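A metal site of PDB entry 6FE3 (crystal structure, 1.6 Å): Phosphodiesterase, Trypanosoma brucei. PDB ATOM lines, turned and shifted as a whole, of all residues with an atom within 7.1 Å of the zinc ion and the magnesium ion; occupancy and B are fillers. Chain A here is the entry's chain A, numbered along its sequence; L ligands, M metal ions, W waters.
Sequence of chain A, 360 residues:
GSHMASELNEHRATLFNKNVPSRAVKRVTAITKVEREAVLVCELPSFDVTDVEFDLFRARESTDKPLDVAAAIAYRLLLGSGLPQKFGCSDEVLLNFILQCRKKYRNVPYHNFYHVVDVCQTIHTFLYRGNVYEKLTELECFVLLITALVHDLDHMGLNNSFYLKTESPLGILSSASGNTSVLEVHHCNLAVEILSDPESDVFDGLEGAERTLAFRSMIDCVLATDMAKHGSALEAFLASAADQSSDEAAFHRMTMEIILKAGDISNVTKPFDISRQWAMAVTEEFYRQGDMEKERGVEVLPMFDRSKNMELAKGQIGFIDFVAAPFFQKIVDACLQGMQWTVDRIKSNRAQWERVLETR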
ATOM      1  N   TYR A 110      21.040  33.789  16.022  1.00  0.00           N
ATOM      2  CA  TYR A 110      21.303  32.532  15.283  1.00  0.00           C
ATOM      3  C   TYR A 110      21.982  31.442  16.163  1.00  0.00           C
ATOM      4  O   TYR A 110      21.431  30.339  16.303  1.00  0.00           O
ATOM      5  CB  TYR A 110      22.109  32.750  14.061  1.00  0.00           C
ATOM      6  CG  TYR A 110      22.339  31.500  13.274  1.00  0.00           C
ATOM      7  CD1 TYR A 110      21.441  31.041  12.337  1.00  0.00           C
ATOM      8  CD2 TYR A 110      23.499  30.759  13.448  1.00  0.00           C
ATOM      9  CE1 TYR A 110      21.652  29.891  11.607  1.00  0.00           C
ATOM     10  CE2 TYR A 110      23.720  29.593  12.730  1.00  0.00           C
ATOM     11  CZ  TYR A 110      22.787  29.134  11.826  1.00  0.00           C
ATOM     12  OH  TYR A 110      22.973  27.992  11.059  1.00  0.00           O
ATOM     13  N   HIS A 111      23.102  31.818  16.772  1.00  0.00           N
ATOM     14  CA  HIS A 111      23.874  30.848  17.629  1.00  0.00           C
ATOM     15  C   HIS A 111      23.346  30.725  19.057  1.00  0.00           C
ATOM     16  O   HIS A 111      24.098  30.837  20.032  1.00  0.00           O
ATOM     17  CB  HIS A 111      25.350  31.201  17.622  1.00  0.00           C
ATOM     18  CG  HIS A 111      26.017  30.983  16.295  1.00  0.00           C
ATOM     19  ND1 HIS A 111      26.339  32.003  15.424  1.00  0.00           N
ATOM     20  CD2 HIS A 111      26.433  29.846  15.700  1.00  0.00           C
ATOM     21  CE1 HIS A 111      26.869  31.491  14.334  1.00  0.00           C
ATOM     22  NE2 HIS A 111      26.975  30.174  14.482  1.00  0.00           N
ATOM     23  N   HIS A 115      19.694  26.629  17.352  1.00  0.00           N
ATOM     24  CA  HIS A 115      20.659  26.157  16.354  1.00  0.00           C
ATOM     25  C   HIS A 115      21.239  24.794  16.713  1.00  0.00           C
ATOM     26  O   HIS A 115      21.377  23.927  15.816  1.00  0.00           O
ATOM     27  CB  HIS A 115      21.771  27.176  16.172  1.00  0.00           C
ATOM     28  CG  HIS A 115      22.958  26.660  15.428  1.00  0.00           C
ATOM     29  ND1 HIS A 115      22.945  26.303  14.094  1.00  0.00           N
ATOM     30  CD2 HIS A 115      24.239  26.502  15.864  1.00  0.00           C
ATOM     31  CE1 HIS A 115      24.183  25.913  13.766  1.00  0.00           C
ATOM     32  NE2 HIS A 115      24.981  26.044  14.814  1.00  0.00           N
ATOM     33  N   VAL A 116      21.555  24.589  17.977  1.00  0.00           N
ATOM     34  CA  VAL A 116      22.239  23.295  18.327  1.00  0.00           C
ATOM     35  C   VAL A 116      21.286  22.175  18.332  1.00  0.00           C
ATOM     36  O   VAL A 116      21.611  21.029  17.962  1.00  0.00           O
ATOM     37  CB  VAL A 116      23.127  23.391  19.595  1.00  0.00           C
ATOM     38  CG1 VAL A 116      24.148  24.493  19.441  1.00  0.00           C
ATOM     39  CG2 VAL A 116      22.327  23.622  20.882  1.00  0.00           C
ATOM     40  N   VAL A 119      20.905  21.313  14.804  1.00  0.00           N
ATOM     41  CA  VAL A 119      22.067  20.497  14.302  1.00  0.00           C
ATOM     42  C   VAL A 119      21.933  19.047  14.767  1.00  0.00           C
ATOM     43  O   VAL A 119      22.227  18.131  13.993  1.00  0.00           O
ATOM     44  CB  VAL A 119      23.417  21.174  14.701  1.00  0.00           C
ATOM     45  CG1 VAL A 119      24.605  20.235  14.441  1.00  0.00           C
ATOM     46  CG2 VAL A 119      23.626  22.504  13.982  1.00  0.00           C
ATOM     47  N   ALA A 148      26.567  17.664  18.977  1.00  0.00           N
ATOM     48  CA  ALA A 148      25.738  18.723  18.408  1.00  0.00           C
ATOM     49  C   ALA A 148      25.302  19.723  19.454  1.00  0.00           C
ATOM     50  O   ALA A 148      25.278  20.929  19.202  1.00  0.00           O
ATOM     51  CB  ALA A 148      24.565  18.077  17.692  1.00  0.00           C
ATOM     52  N   HIS A 151      28.289  22.169  20.646  1.00  0.00           N
ATOM     53  CA  HIS A 151      29.302  22.559  19.707  1.00  0.00           C
ATOM     54  C   HIS A 151      29.441  24.080  19.550  1.00  0.00           C
ATOM     55  O   HIS A 151      30.409  24.566  18.985  1.00  0.00           O
ATOM     56  CB  HIS A 151      29.091  21.873  18.350  1.00  0.00           C
ATOM     57  CG  HIS A 151      28.176  22.636  17.436  1.00  0.00           C
ATOM     58  ND1 HIS A 151      26.805  22.440  17.454  1.00  0.00           N
ATOM     59  CD2 HIS A 151      28.431  23.591  16.519  1.00  0.00           C
ATOM     60  CE1 HIS A 151      26.267  23.282  16.576  1.00  0.00           C
ATOM     61  NE2 HIS A 151      27.233  23.956  15.972  1.00  0.00           N
ATOM     62  N   ASP A 152      28.441  24.817  20.046  1.00  0.00           N
ATOM     63  CA  ASP A 152      28.476  26.311  20.117  1.00  0.00           C
ATOM     64  C   ASP A 152      28.284  26.949  21.488  1.00  0.00           C
ATOM     65  O   ASP A 152      27.875  28.086  21.597  1.00  0.00           O
ATOM     66  CB  ASP A 152      27.438  26.856  19.146  1.00  0.00           C
ATOM     67  CG  ASP A 152      27.976  26.914  17.687  1.00  0.00           C
ATOM     68  OD1 ASP A 152      29.171  27.157  17.430  1.00  0.00           O
ATOM     69  OD2 ASP A 152      27.107  26.725  16.791  1.00  0.00           O
ATOM     70  N   LEU A 153      28.591  26.203  22.536  1.00  0.00           N
ATOM     71  CA  LEU A 153      28.297  26.654  23.877  1.00  0.00           C
ATOM     72  C   LEU A 153      28.859  28.064  24.133  1.00  0.00           C
ATOM     73  O   LEU A 153      30.019  28.298  23.940  1.00  0.00           O
ATOM     74  CB  LEU A 153      28.940  25.778  24.973  1.00  0.00           C
ATOM     75  CG  LEU A 153      28.268  24.411  25.147  1.00  0.00           C
ATOM     76  CD1 LEU A 153      29.200  23.440  25.854  1.00  0.00           C
ATOM     77  CD2 LEU A 153      26.905  24.527  25.856  1.00  0.00           C
ATOM     78  N   HIS A 155      28.331  30.884  22.693  1.00  0.00           N
ATOM     79  CA  HIS A 155      28.500  31.795  21.589  1.00  0.00           C
ATOM     80  C   HIS A 155      27.859  33.125  21.915  1.00  0.00           C
ATOM     81  O   HIS A 155      26.743  33.131  22.392  1.00  0.00           O
ATOM     82  CB  HIS A 155      27.832  31.200  20.312  1.00  0.00           C
ATOM     83  CG  HIS A 155      28.461  31.657  19.055  1.00  0.00           C
ATOM     84  ND1 HIS A 155      28.306  32.947  18.576  1.00  0.00           N
ATOM     85  CD2 HIS A 155      29.198  30.986  18.138  1.00  0.00           C
ATOM     86  CE1 HIS A 155      28.934  33.044  17.409  1.00  0.00           C
ATOM     87  NE2 HIS A 155      29.520  31.884  17.154  1.00  0.00           N
ATOM     88  N   LEU A 183      36.585  30.578  19.372  1.00  0.00           N
ATOM     89  CA  LEU A 183      35.344  30.106  19.921  1.00  0.00           C
ATOM     90  C   LEU A 183      35.326  28.590  20.158  1.00  0.00           C
ATOM     91  O   LEU A 183      34.783  28.133  21.138  1.00  0.00           O
ATOM     92  CB  LEU A 183      34.180  30.505  19.037  1.00  0.00           C
ATOM     93  CG  LEU A 183      33.843  31.995  19.167  1.00  0.00           C
ATOM     94  CD1 LEU A 183      32.824  32.283  18.138  1.00  0.00           C
ATOM     95  CD2 LEU A 183      33.327  32.375  20.569  1.00  0.00           C
ATOM     96  N   GLU A 184      35.804  27.851  19.181  1.00  0.00           N
ATOM     97  CA  GLU A 184      35.731  26.397  19.229  1.00  0.00           C
ATOM     98  C   GLU A 184      36.455  25.833  20.439  1.00  0.00           C
ATOM     99  O   GLU A 184      35.943  24.943  21.114  1.00  0.00           O
ATOM    100  CB  GLU A 184      36.236  25.762  17.923  1.00  0.00           C
ATOM    101  CG  GLU A 184      35.361  26.102  16.684  1.00  0.00           C
ATOM    102  CD  GLU A 184      35.507  27.507  16.113  1.00  0.00           C
ATOM    103  OE1 GLU A 184      36.473  28.223  16.432  1.00  0.00           O
ATOM    104  OE2 GLU A 184      34.591  27.912  15.325  1.00  0.00           O
ATOM    105  N   HIS A 187      34.117  26.561  23.348  1.00  0.00           N
ATOM    106  CA  HIS A 187      33.028  25.620  23.452  1.00  0.00           C
ATOM    107  C   HIS A 187      33.491  24.301  24.062  1.00  0.00           C
ATOM    108  O   HIS A 187      32.742  23.696  24.883  1.00  0.00           O
ATOM    109  CB  HIS A 187      32.415  25.316  22.054  1.00  0.00           C
ATOM    110  CG  HIS A 187      32.057  26.529  21.229  1.00  0.00           C
ATOM    111  ND1 HIS A 187      31.443  27.652  21.758  1.00  0.00           N
ATOM    112  CD2 HIS A 187      32.218  26.773  19.900  1.00  0.00           C
ATOM    113  CE1 HIS A 187      31.243  28.517  20.781  1.00  0.00           C
ATOM    114  NE2 HIS A 187      31.661  27.997  19.643  1.00  0.00           N
ATOM    115  N   VAL A 222      34.173  19.331  17.394  1.00  0.00           N
ATOM    116  CA  VAL A 222      33.957  20.738  17.682  1.00  0.00           C
ATOM    117  C   VAL A 222      35.055  21.626  17.058  1.00  0.00           C
ATOM    118  O   VAL A 222      34.756  22.633  16.415  1.00  0.00           O
ATOM    119  CB  VAL A 222      33.777  21.044  19.204  1.00  0.00           C
ATOM    120  CG1 VAL A 222      33.649  22.541  19.478  1.00  0.00           C
ATOM    121  CG2 VAL A 222      32.605  20.308  19.726  1.00  0.00           C
ATOM    122  N   THR A 225      34.672  22.423  13.376  1.00  0.00           N
ATOM    123  CA  THR A 225      33.601  23.350  12.933  1.00  0.00           C
ATOM    124  C   THR A 225      34.108  24.728  12.590  1.00  0.00           C
ATOM    125  O   THR A 225      33.304  25.525  12.055  1.00  0.00           O
ATOM    126  CB  THR A 225      32.422  23.468  13.896  1.00  0.00           C
ATOM    127  OG1 THR A 225      32.848  23.952  15.178  1.00  0.00           O
ATOM    128  CG2 THR A 225      31.707  22.143  14.048  1.00  0.00           C
ATOM    129  N   ASP A 226      35.375  25.059  12.890  1.00  0.00           N
ATOM    130  CA  ASP A 226      35.936  26.361  12.486  1.00  0.00           C
ATOM    131  C   ASP A 226      35.965  26.464  10.945  1.00  0.00           C
ATOM    132  O   ASP A 226      36.668  25.723  10.331  1.00  0.00           O
ATOM    133  CB  ASP A 226      37.320  26.512  13.065  1.00  0.00           C
ATOM    134  CG  ASP A 226      37.975  27.877  12.760  1.00  0.00           C
ATOM    135  OD1 ASP A 226      37.491  28.625  11.918  1.00  0.00           O
ATOM    136  OD2 ASP A 226      39.087  28.142  13.349  1.00  0.00           O
ATOM    137  N   LEU A 260      29.375  16.524  11.571  1.00  0.00           N
ATOM    138  CA  LEU A 260      29.056  17.718  12.370  1.00  0.00           C
ATOM    139  C   LEU A 260      29.173  18.943  11.525  1.00  0.00           C
ATOM    140  O   LEU A 260      28.287  19.810  11.576  1.00  0.00           O
ATOM    141  CB  LEU A 260      29.953  17.834  13.588  1.00  0.00           C
ATOM    142  CG  LEU A 260      29.649  19.068  14.456  1.00  0.00           C
ATOM    143  CD1 LEU A 260      28.278  19.086  15.055  1.00  0.00           C
ATOM    144  CD2 LEU A 260      30.623  19.110  15.619  1.00  0.00           C
ATOM    145  N   GLY A 263      26.007  19.170   9.447  1.00  0.00           N
ATOM    146  CA  GLY A 263      24.909  19.663  10.226  1.00  0.00           C
ATOM    147  C   GLY A 263      24.992  21.153  10.379  1.00  0.00           C
ATOM    148  O   GLY A 263      23.951  21.905  10.277  1.00  0.00           O
ATOM    149  N   ASP A 264      26.182  21.600  10.651  1.00  0.00           N
ATOM    150  CA  ASP A 264      26.399  23.047  10.839  1.00  0.00           C
ATOM    151  C   ASP A 264      26.114  23.909   9.593  1.00  0.00           C
ATOM    152  O   ASP A 264      25.655  25.047   9.738  1.00  0.00           O
ATOM    153  CB  ASP A 264      27.868  23.229  11.295  1.00  0.00           C
ATOM    154  CG  ASP A 264      28.051  24.321  12.382  1.00  0.00           C
ATOM    155  OD1 ASP A 264      27.071  24.724  13.001  1.00  0.00           O
ATOM    156  OD2 ASP A 264      29.234  24.737  12.528  1.00  0.00           O
ATOM    157  N   ILE A 265      26.299  23.407   8.369  1.00  0.00           N
ATOM    158  CA  ILE A 265      25.965  24.176   7.149  1.00  0.00           C
ATOM    159  C   ILE A 265      24.743  23.579   6.416  1.00  0.00           C
ATOM    160  O   ILE A 265      24.592  23.761   5.203  1.00  0.00           O
ATOM    161  CB  ILE A 265      27.163  24.327   6.217  1.00  0.00           C
ATOM    162  CG1 ILE A 265      27.730  22.988   5.795  1.00  0.00           C
ATOM    163  CG2 ILE A 265      28.262  25.104   6.950  1.00  0.00           C
ATOM    164  CD1 ILE A 265      28.672  23.102   4.640  1.00  0.00           C
HETATM  165  O1  LIG L   1      22.811  30.883   5.550  1.00  0.00           O
HETATM  166  C1  LIG L   1      29.095  30.404  10.321  1.00  0.00           C
HETATM  167  N1  LIG L   1      31.834  32.578   4.607  1.00  0.00           N
HETATM  168  C2  LIG L   1      32.099  31.162   4.917  1.00  0.00           C
HETATM  169  C3  LIG L   1      31.524  33.082   3.383  1.00  0.00           C
HETATM  170  C4  LIG L   1      31.096  30.638   5.939  1.00  0.00           C
HETATM  171  C5  LIG L   1      31.036  31.529   7.169  1.00  0.00           C
HETATM  172  C6  LIG L   1      27.751  30.560   8.218  1.00  0.00           C
HETATM  173  C7  LIG L   1      31.461  32.091   2.232  1.00  0.00           C
HETATM  174  C8  LIG L   1      32.396  33.131   0.185  1.00  0.00           C
HETATM  175  C9  LIG L   1      32.182  33.849  -1.122  1.00  0.00           C
HETATM  176  C10 LIG L   1      30.865  35.806  -0.272  1.00  0.00           C
HETATM  177  N2  LIG L   1      31.244  32.774   0.940  1.00  0.00           N
HETATM  178  C11 LIG L   1      30.850  34.597  -1.223  1.00  0.00           C
HETATM  179  C12 LIG L   1      30.619  35.075  -2.665  1.00  0.00           C
HETATM  180  C13 LIG L   1      24.111  29.875   7.396  1.00  0.00           C
HETATM  181  C14 LIG L   1      25.333  29.826   8.061  1.00  0.00           C
HETATM  182  C15 LIG L   1      26.405  30.595   7.612  1.00  0.00           C
HETATM  183  N3  LIG L   1      29.979  31.120   8.132  1.00  0.00           N
HETATM  184  O2  LIG L   1      33.515  32.917   0.605  1.00  0.00           O
HETATM  185  O3  LIG L   1      31.252  34.279   3.191  1.00  0.00           O
HETATM  186  C16 LIG L   1      23.946  30.694   6.284  1.00  0.00           C
HETATM  187  C17 LIG L   1      29.379  29.522  11.531  1.00  0.00           C
HETATM  188  C18 LIG L   1      29.673  28.101  11.141  1.00  0.00           C
HETATM  189  C19 LIG L   1      25.016  33.493   4.401  1.00  0.00           C
HETATM  190  C20 LIG L   1      25.020  31.468   5.813  1.00  0.00           C
HETATM  191  C21 LIG L   1      21.800  30.004   5.565  1.00  0.00           C
HETATM  192  C22 LIG L   1      29.267  27.567   9.992  1.00  0.00           C
HETATM  193  C23 LIG L   1      28.479  28.307   8.969  1.00  0.00           C
HETATM  194  C24 LIG L   1      28.017  29.695   9.443  1.00  0.00           C
HETATM  195  C25 LIG L   1      26.257  31.365   6.440  1.00  0.00           C
HETATM  196  N4  LIG L   1      28.690  31.216   7.622  1.00  0.00           N
HETATM  197  F1  LIG L   1      22.304  28.755   5.349  1.00  0.00           F
HETATM  198  F2  LIG L   1      21.220  30.006   6.795  1.00  0.00           F
HETATM  199  O4  LIG L   1      24.772  32.188   4.673  1.00  0.00           O
HETATM  200  F3  LIG L   1      26.121  33.903   5.012  1.00  0.00           F
HETATM  201  F4  LIG L   1      25.334  33.590   3.096  1.00  0.00           F
HETATM  202  C26 LIG L   1      30.274  30.724   9.427  1.00  0.00           C
HETATM  203  O5  LIG L   1      31.429  30.579   9.796  1.00  0.00           O
HETATM  204  C27 LIG L   1      30.846  32.998   6.812  1.00  0.00           C
HETATM  205  C28 LIG L   1      31.884  33.444   5.804  1.00  0.00           C
HETATM  206  C29 LIG L   1      29.922  33.139   0.608  1.00  0.00           C
HETATM  207  O6  LIG L   1      29.027  33.183   1.438  1.00  0.00           O
HETATM  208  C30 LIG L   1      29.744  33.622  -0.796  1.00  0.00           C
HETATM  209 ZN    ZN M   1      27.100  25.816  14.818  1.00  0.00          ZN
HETATM  210 MG    MG M   2      30.506  27.234  15.811  1.00  0.00          MG
HETATM  211  O   HOH W   1      31.644  28.637  16.928  1.00  0.00           O
HETATM  212  O   HOH W   2      29.173  26.116  14.682  1.00  0.00           O
HETATM  213  O   HOH W   3      29.628  28.918  14.861  1.00  0.00           O
HETATM  214  O   HOH W   4      27.155  27.593  13.465  1.00  0.00           O
HETATM  215  O   HOH W   5      32.126  27.145  14.447  1.00  0.00           O
HETATM  216  O   HOH W   6      31.462  25.631  16.766  1.00  0.00           O
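The nearest printed residue that does not touch the magnesium ion is His 187 (4.1 Å).
Along chain A the residues within 4 Å of the zinc ion span positions 115 to 264.
The zinc ion is bound by water W2 (2.1 Å). OD1 of Asp 264 is bound to the zinc ion (2.1 Å). The zinc ion is bound by NE2 of His 115, 2.1 Å away. OD2 of Asp 152 binds the zinc ion, at 2.2 Å. The zinc ion is bound by NE2 of His 151, at 2.2 Å. Water W4 binds the zinc ion (2.2 Å). The zinc ion has six donor atoms within binding distance.
The side-chain carboxylate of Asp 152 sits close to a ring nitrogen (NE2) of His 187 (3.4 Å). ND1 of His 115 lies within hydrogen-bond range of OH of Tyr 110, 3.5 Å away. The backbone carbonyl oxygen of Ala 148 is in hydrogen-bond range of a ring nitrogen (ND1) of His 151, at 2.8 Å.
Water W6 lies within hydrogen-bond range of O of His 151 (2.7 Å) and OG1 of Thr 225 (2.7 Å). Water W1 lies within hydrogen-bond range of a ring nitrogen (NE2) of His 187 (2.8 Å) and the side-chain carboxylate (OE2) of Glu 184 (3.4 Å). Water W5 lies within hydrogen-bond range of the side-chain carboxylate of Glu 184 (2.7 Å) and the backbone carbonyl oxygen of Thr 225 (3.1 Å).
The magnesium ion is bound by water W2 (2.1 Å), water W6 (2.1 Å), OD1 of Asp 152 (2.1 Å), water W5 (2.1 Å), water W3 (2.1 Å) and water W1 (2.1 Å).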
